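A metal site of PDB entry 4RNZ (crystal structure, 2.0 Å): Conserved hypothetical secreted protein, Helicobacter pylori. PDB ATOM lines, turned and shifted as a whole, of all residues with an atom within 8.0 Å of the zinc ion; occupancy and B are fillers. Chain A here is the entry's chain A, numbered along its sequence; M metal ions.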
ATOM      1  N   SER A  30     -26.945  -7.308   5.934  1.00  0.00           N
ATOM      2  CA  SER A  30     -26.140  -6.461   6.795  1.00  0.00           C
ATOM      3  C   SER A  30     -25.157  -7.302   7.623  1.00  0.00           C
ATOM      4  O   SER A  30     -24.074  -6.823   7.970  1.00  0.00           O
ATOM      5  CB  SER A  30     -27.011  -5.592   7.699  1.00  0.00           C
ATOM      6  OG  SER A  30     -27.859  -6.416   8.456  1.00  0.00           O
ATOM      7  N   GLN A  31     -25.533  -8.532   7.925  1.00  0.00           N
ATOM      8  CA  GLN A  31     -24.640  -9.480   8.600  1.00  0.00           C
ATOM      9  C   GLN A  31     -23.434  -9.796   7.705  1.00  0.00           C
ATOM     10  O   GLN A  31     -22.303  -9.754   8.168  1.00  0.00           O
ATOM     11  CB  GLN A  31     -25.370 -10.768   8.980  1.00  0.00           C
ATOM     12  CG  GLN A  31     -26.509 -10.588   9.983  1.00  0.00           C
ATOM     13  CD  GLN A  31     -27.861 -10.275   9.330  1.00  0.00           C
ATOM     14  OE1 GLN A  31     -27.948  -9.975   8.130  1.00  0.00           O
ATOM     15  NE2 GLN A  31     -28.925 -10.319  10.136  1.00  0.00           N
ATOM     16  N   GLU A  34     -21.116  -6.740   7.560  1.00  0.00           N
ATOM     17  CA  GLU A  34     -20.262  -6.666   8.745  1.00  0.00           C
ATOM     18  C   GLU A  34     -19.055  -7.617   8.583  1.00  0.00           C
ATOM     19  O   GLU A  34     -17.912  -7.269   8.846  1.00  0.00           O
ATOM     20  CB  GLU A  34     -21.026  -7.048  10.024  1.00  0.00           C
ATOM     21  CG  GLU A  34     -21.932  -5.967  10.580  1.00  0.00           C
ATOM     22  CD  GLU A  34     -22.303  -6.201  12.059  1.00  0.00           C
ATOM     23  OE1 GLU A  34     -22.674  -5.219  12.731  1.00  0.00           O
ATOM     24  OE2 GLU A  34     -22.231  -7.354  12.555  1.00  0.00           O
ATOM     25  N   LEU A  35     -19.346  -8.811   8.097  1.00  0.00           N
ATOM     26  CA  LEU A  35     -18.328  -9.846   7.879  1.00  0.00           C
ATOM     27  C   LEU A  35     -17.243  -9.308   6.908  1.00  0.00           C
ATOM     28  O   LEU A  35     -16.030  -9.397   7.177  1.00  0.00           O
ATOM     29  CB  LEU A  35     -19.028 -11.101   7.334  1.00  0.00           C
ATOM     30  CG  LEU A  35     -18.792 -12.501   7.860  1.00  0.00           C
ATOM     31  CD1 LEU A  35     -18.688 -12.580   9.374  1.00  0.00           C
ATOM     32  CD2 LEU A  35     -19.897 -13.397   7.324  1.00  0.00           C
ATOM     33  N   SER A 201     -28.855  -8.764  20.258  1.00  0.00           N
ATOM     34  CA  SER A 201     -29.601  -9.208  19.060  1.00  0.00           C
ATOM     35  C   SER A 201     -28.846 -10.268  18.253  1.00  0.00           C
ATOM     36  O   SER A 201     -29.430 -10.942  17.421  1.00  0.00           O
ATOM     37  CB  SER A 201     -29.948  -8.033  18.152  1.00  0.00           C
ATOM     38  OG  SER A 201     -28.786  -7.320  17.828  1.00  0.00           O
ATOM     39  N   SER A 202     -27.560 -10.423  18.478  1.00  0.00           N
ATOM     40  CA  SER A 202     -26.813 -11.455  17.786  1.00  0.00           C
ATOM     41  C   SER A 202     -25.509 -11.709  18.525  1.00  0.00           C
ATOM     42  O   SER A 202     -24.654 -10.831  18.585  1.00  0.00           O
ATOM     43  CB  SER A 202     -26.533 -11.046  16.334  1.00  0.00           C
ATOM     44  OG  SER A 202     -25.965 -12.140  15.640  1.00  0.00           O
ATOM     45  N   PRO A 203     -25.357 -12.914  19.091  1.00  0.00           N
ATOM     46  CA  PRO A 203     -24.122 -13.178  19.803  1.00  0.00           C
ATOM     47  C   PRO A 203     -22.963 -13.524  18.870  1.00  0.00           C
ATOM     48  O   PRO A 203     -23.134 -13.600  17.653  1.00  0.00           O
ATOM     49  CB  PRO A 203     -24.489 -14.380  20.686  1.00  0.00           C
ATOM     50  CG  PRO A 203     -25.479 -15.131  19.864  1.00  0.00           C
ATOM     51  CD  PRO A 203     -26.258 -14.080  19.110  1.00  0.00           C
ATOM     52  N   PHE A 204     -21.810 -13.734  19.452  1.00  0.00           N
ATOM     53  CA  PHE A 204     -20.639 -14.166  18.730  1.00  0.00           C
ATOM     54  C   PHE A 204     -20.849 -15.561  18.242  1.00  0.00           C
ATOM     55  O   PHE A 204     -21.355 -16.398  18.972  1.00  0.00           O
ATOM     56  CB  PHE A 204     -19.428 -14.145  19.661  1.00  0.00           C
ATOM     57  CG  PHE A 204     -18.140 -14.521  18.996  1.00  0.00           C
ATOM     58  CD1 PHE A 204     -17.751 -15.857  18.874  1.00  0.00           C
ATOM     59  CD2 PHE A 204     -17.319 -13.540  18.450  1.00  0.00           C
ATOM     60  CE1 PHE A 204     -16.551 -16.210  18.256  1.00  0.00           C
ATOM     61  CE2 PHE A 204     -16.110 -13.884  17.814  1.00  0.00           C
ATOM     62  CZ  PHE A 204     -15.730 -15.216  17.722  1.00  0.00           C
ATOM     63  N   PRO A 218     -21.537 -17.145  10.733  1.00  0.00           N
ATOM     64  CA  PRO A 218     -20.420 -16.605  11.525  1.00  0.00           C
ATOM     65  C   PRO A 218     -20.609 -15.129  11.853  1.00  0.00           C
ATOM     66  O   PRO A 218     -20.851 -14.342  10.961  1.00  0.00           O
ATOM     67  CB  PRO A 218     -19.203 -16.769  10.611  1.00  0.00           C
ATOM     68  CG  PRO A 218     -19.667 -17.572   9.456  1.00  0.00           C
ATOM     69  CD  PRO A 218     -21.144 -17.372   9.335  1.00  0.00           C
ATOM     70  N   HIS A 219     -20.458 -14.767  13.117  1.00  0.00           N
ATOM     71  CA  HIS A 219     -20.570 -13.361  13.542  1.00  0.00           C
ATOM     72  C   HIS A 219     -19.449 -13.024  14.520  1.00  0.00           C
ATOM     73  O   HIS A 219     -19.401 -13.580  15.612  1.00  0.00           O
ATOM     74  CB  HIS A 219     -21.943 -13.107  14.174  1.00  0.00           C
ATOM     75  CG  HIS A 219     -22.171 -11.705  14.631  1.00  0.00           C
ATOM     76  ND1 HIS A 219     -22.596 -11.390  15.908  1.00  0.00           N
ATOM     77  CD2 HIS A 219     -22.006 -10.520  13.994  1.00  0.00           C
ATOM     78  CE1 HIS A 219     -22.716 -10.085  16.025  1.00  0.00           C
ATOM     79  NE2 HIS A 219     -22.376  -9.537  14.869  1.00  0.00           N
ATOM     80  N   TYR A 220     -18.539 -12.146  14.098  1.00  0.00           N
ATOM     81  CA  TYR A 220     -17.296 -11.953  14.812  1.00  0.00           C
ATOM     82  C   TYR A 220     -17.360 -10.777  15.817  1.00  0.00           C
ATOM     83  O   TYR A 220     -16.433  -9.986  15.931  1.00  0.00           O
ATOM     84  CB  TYR A 220     -16.132 -11.801  13.835  1.00  0.00           C
ATOM     85  CG  TYR A 220     -15.801 -13.067  13.051  1.00  0.00           C
ATOM     86  CD1 TYR A 220     -15.838 -14.320  13.657  1.00  0.00           C
ATOM     87  CD2 TYR A 220     -15.415 -12.995  11.713  1.00  0.00           C
ATOM     88  CE1 TYR A 220     -15.516 -15.473  12.938  1.00  0.00           C
ATOM     89  CE2 TYR A 220     -15.092 -14.147  10.983  1.00  0.00           C
ATOM     90  CZ  TYR A 220     -15.151 -15.381  11.611  1.00  0.00           C
ATOM     91  OH  TYR A 220     -14.818 -16.525  10.924  1.00  0.00           O
ATOM     92  N   GLY A 221     -18.454 -10.706  16.566  1.00  0.00           N
ATOM     93  CA  GLY A 221     -18.644  -9.696  17.600  1.00  0.00           C
ATOM     94  C   GLY A 221     -19.973  -9.977  18.274  1.00  0.00           C
ATOM     95  O   GLY A 221     -20.558 -11.015  18.070  1.00  0.00           O
ATOM     96  N   VAL A 222     -20.407  -9.053  19.116  1.00  0.00           N
ATOM     97  CA  VAL A 222     -21.702  -9.132  19.769  1.00  0.00           C
ATOM     98  C   VAL A 222     -22.455  -7.905  19.294  1.00  0.00           C
ATOM     99  O   VAL A 222     -21.919  -6.805  19.310  1.00  0.00           O
ATOM    100  CB  VAL A 222     -21.575  -9.064  21.306  1.00  0.00           C
ATOM    101  CG1 VAL A 222     -22.954  -9.055  21.955  1.00  0.00           C
ATOM    102  CG2 VAL A 222     -20.739 -10.210  21.818  1.00  0.00           C
ATOM    103  N   ASP A 223     -23.682  -8.112  18.842  1.00  0.00           N
ATOM    104  CA  ASP A 223     -24.573  -7.014  18.481  1.00  0.00           C
ATOM    105  C   ASP A 223     -25.460  -6.712  19.671  1.00  0.00           C
ATOM    106  O   ASP A 223     -26.210  -7.564  20.148  1.00  0.00           O
ATOM    107  CB  ASP A 223     -25.420  -7.361  17.249  1.00  0.00           C
ATOM    108  CG  ASP A 223     -24.608  -7.380  15.980  1.00  0.00           C
ATOM    109  OD1 ASP A 223     -23.451  -6.905  15.987  1.00  0.00           O
ATOM    110  OD2 ASP A 223     -25.090  -7.872  14.957  1.00  0.00           O
ATOM    111  N   TYR A 224     -25.332  -5.483  20.170  1.00  0.00           N
ATOM    112  CA  TYR A 224     -26.087  -5.035  21.329  1.00  0.00           C
ATOM    113  C   TYR A 224     -27.147  -4.107  20.811  1.00  0.00           C
ATOM    114  O   TYR A 224     -26.821  -3.052  20.280  1.00  0.00           O
ATOM    115  CB  TYR A 224     -25.210  -4.221  22.273  1.00  0.00           C
ATOM    116  CG  TYR A 224     -24.168  -4.975  23.086  1.00  0.00           C
ATOM    117  CD1 TYR A 224     -24.520  -5.809  24.152  1.00  0.00           C
ATOM    118  CD2 TYR A 224     -22.806  -4.800  22.825  1.00  0.00           C
ATOM    119  CE1 TYR A 224     -23.564  -6.461  24.902  1.00  0.00           C
ATOM    120  CE2 TYR A 224     -21.850  -5.438  23.578  1.00  0.00           C
ATOM    121  CZ  TYR A 224     -22.222  -6.263  24.623  1.00  0.00           C
ATOM    122  OH  TYR A 224     -21.242  -6.890  25.348  1.00  0.00           O
ATOM    123  N   GLY A 248     -19.742  -1.305   5.928  1.00  0.00           N
ATOM    124  CA  GLY A 248     -20.252  -2.482   6.632  1.00  0.00           C
ATOM    125  C   GLY A 248     -20.270  -2.258   8.138  1.00  0.00           C
ATOM    126  O   GLY A 248     -21.081  -2.847   8.839  1.00  0.00           O
ATOM    127  N   TYR A 249     -19.396  -1.391   8.633  1.00  0.00           N
ATOM    128  CA  TYR A 249     -19.383  -1.018  10.040  1.00  0.00           C
ATOM    129  C   TYR A 249     -19.921   0.387  10.282  1.00  0.00           C
ATOM    130  O   TYR A 249     -20.230   0.740  11.431  1.00  0.00           O
ATOM    131  CB  TYR A 249     -17.968  -1.052  10.574  1.00  0.00           C
ATOM    132  CG  TYR A 249     -17.427  -2.373  11.021  1.00  0.00           C
ATOM    133  CD1 TYR A 249     -18.249  -3.405  11.469  1.00  0.00           C
ATOM    134  CD2 TYR A 249     -16.045  -2.564  11.086  1.00  0.00           C
ATOM    135  CE1 TYR A 249     -17.720  -4.598  11.913  1.00  0.00           C
ATOM    136  CE2 TYR A 249     -15.508  -3.748  11.522  1.00  0.00           C
ATOM    137  CZ  TYR A 249     -16.350  -4.769  11.939  1.00  0.00           C
ATOM    138  OH  TYR A 249     -15.843  -5.955  12.392  1.00  0.00           O
ATOM    139  N   ALA A 265     -18.578  -0.544  16.527  1.00  0.00           N
ATOM    140  CA  ALA A 265     -19.067  -0.127  15.223  1.00  0.00           C
ATOM    141  C   ALA A 265     -20.548   0.258  15.207  1.00  0.00           C
ATOM    142  O   ALA A 265     -21.319  -0.107  16.093  1.00  0.00           O
ATOM    143  CB  ALA A 265     -18.815  -1.231  14.191  1.00  0.00           C
ATOM    144  N   HIS A 266     -20.885   0.964  14.125  1.00  0.00           N
ATOM    145  CA  HIS A 266     -22.194   1.521  13.831  1.00  0.00           C
ATOM    146  C   HIS A 266     -22.492   2.775  14.647  1.00  0.00           C
ATOM    147  O   HIS A 266     -23.638   3.033  14.973  1.00  0.00           O
ATOM    148  CB  HIS A 266     -23.302   0.480  13.994  1.00  0.00           C
ATOM    149  CG  HIS A 266     -23.108  -0.749  13.153  1.00  0.00           C
ATOM    150  ND1 HIS A 266     -23.145  -0.711  11.780  1.00  0.00           N
ATOM    151  CD2 HIS A 266     -22.863  -2.032  13.493  1.00  0.00           C
ATOM    152  CE1 HIS A 266     -22.927  -1.926  11.307  1.00  0.00           C
ATOM    153  NE2 HIS A 266     -22.744  -2.737  12.324  1.00  0.00           N
ATOM    154  N   HIS A 299     -27.881  -0.570  16.734  1.00  0.00           N
ATOM    155  CA  HIS A 299     -27.107  -1.465  17.600  1.00  0.00           C
ATOM    156  C   HIS A 299     -25.634  -1.099  17.606  1.00  0.00           C
ATOM    157  O   HIS A 299     -25.154  -0.417  16.711  1.00  0.00           O
ATOM    158  CB  HIS A 299     -27.287  -2.947  17.174  1.00  0.00           C
ATOM    159  CG  HIS A 299     -26.694  -3.261  15.829  1.00  0.00           C
ATOM    160  ND1 HIS A 299     -27.241  -2.810  14.646  1.00  0.00           N
ATOM    161  CD2 HIS A 299     -25.605  -3.992  15.476  1.00  0.00           C
ATOM    162  CE1 HIS A 299     -26.510  -3.235  13.630  1.00  0.00           C
ATOM    163  NE2 HIS A 299     -25.515  -3.957  14.111  1.00  0.00           N
ATOM    164  N   LEU A 300     -24.935  -1.518  18.652  1.00  0.00           N
ATOM    165  CA  LEU A 300     -23.470  -1.459  18.707  1.00  0.00           C
ATOM    166  C   LEU A 300     -22.971  -2.838  18.324  1.00  0.00           C
ATOM    167  O   LEU A 300     -23.358  -3.832  18.940  1.00  0.00           O
ATOM    168  CB  LEU A 300     -22.997  -1.112  20.114  1.00  0.00           C
ATOM    169  CG  LEU A 300     -21.501  -1.315  20.368  1.00  0.00           C
ATOM    170  CD1 LEU A 300     -20.707  -0.340  19.505  1.00  0.00           C
ATOM    171  CD2 LEU A 300     -21.219  -1.146  21.838  1.00  0.00           C
ATOM    172  N   HIS A 301     -22.108  -2.923  17.323  1.00  0.00           N
ATOM    173  CA  HIS A 301     -21.360  -4.137  17.082  1.00  0.00           C
ATOM    174  C   HIS A 301     -20.061  -4.007  17.882  1.00  0.00           C
ATOM    175  O   HIS A 301     -19.284  -3.076  17.660  1.00  0.00           O
ATOM    176  CB  HIS A 301     -21.074  -4.322  15.590  1.00  0.00           C
ATOM    177  CG  HIS A 301     -20.130  -5.440  15.305  1.00  0.00           C
ATOM    178  ND1 HIS A 301     -20.553  -6.667  14.855  1.00  0.00           N
ATOM    179  CD2 HIS A 301     -18.789  -5.536  15.461  1.00  0.00           C
ATOM    180  CE1 HIS A 301     -19.509  -7.473  14.741  1.00  0.00           C
ATOM    181  NE2 HIS A 301     -18.424  -6.809  15.093  1.00  0.00           N
ATOM    182  N   PHE A 302     -19.839  -4.929  18.826  1.00  0.00           N
ATOM    183  CA  PHE A 302     -18.682  -4.944  19.708  1.00  0.00           C
ATOM    184  C   PHE A 302     -17.830  -6.164  19.392  1.00  0.00           C
ATOM    185  O   PHE A 302     -18.289  -7.299  19.579  1.00  0.00           O
ATOM    186  CB  PHE A 302     -19.099  -4.943  21.195  1.00  0.00           C
ATOM    187  CG  PHE A 302     -17.937  -5.003  22.193  1.00  0.00           C
ATOM    188  CD1 PHE A 302     -16.822  -4.181  22.072  1.00  0.00           C
ATOM    189  CD2 PHE A 302     -17.971  -5.889  23.254  1.00  0.00           C
ATOM    190  CE1 PHE A 302     -15.782  -4.229  22.991  1.00  0.00           C
ATOM    191  CE2 PHE A 302     -16.946  -5.938  24.182  1.00  0.00           C
ATOM    192  CZ  PHE A 302     -15.836  -5.121  24.040  1.00  0.00           C
ATOM    193  N   GLY A 303     -16.634  -5.926  18.885  1.00  0.00           N
ATOM    194  CA  GLY A 303     -15.732  -7.007  18.490  1.00  0.00           C
ATOM    195  C   GLY A 303     -14.435  -7.033  19.290  1.00  0.00           C
ATOM    196  O   GLY A 303     -13.889  -5.987  19.644  1.00  0.00           O
HETATM  197 ZN    ZN M   1     -22.311  -7.587  14.531  1.00  0.00          ZN
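Of the 24 residues printed, 4 come within 4 Å of the zinc ion. The nearest printed residue that does not touch the zinc ion is Val 222 (4.8 Å).
The backbone NH (N) of Asp 223 sits at hydrogen-bond distance from the backbone carbonyl oxygen (O) of Ser 202 (2.9 Å). The backbone NH (N) of Ser 201 lies within hydrogen-bond range of the backbone carbonyl oxygen (O) of Asp 223 (2.9 Å). A ring nitrogen (ND1) of His 219 is in hydrogen-bond range of the backbone carbonyl oxygen (O) of Gly 221, 3.0 Å away. ND1 of His 219 lies close to O of Ser 202, at 3.4 Å. O of Pro 203 is in hydrogen-bond range of ND1 of His 219, 2.9 Å away. OE1 of Glu 34 lies within hydrogen-bond range of NE2 of His 299. OE1 of Glu 34 lies within hydrogen-bond range of NE2 of His 266 (2.5 Å). The backbone carbonyl oxygen (O) of His 301 lies within hydrogen-bond range of the backbone NH (N) of Ala 265, 2.9 Å away.
The zinc ion is bound by OD1 of Asp 223 (2.0 Å), NE2 of His 219 (2.0 Å), OE2 of Glu 34 (2.0 Å) and ND1 of His 301 (2.0 Å). Slightly farther from the zinc ion lies the side-chain carboxylate (OD2) of Asp 223 (2.8 Å).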
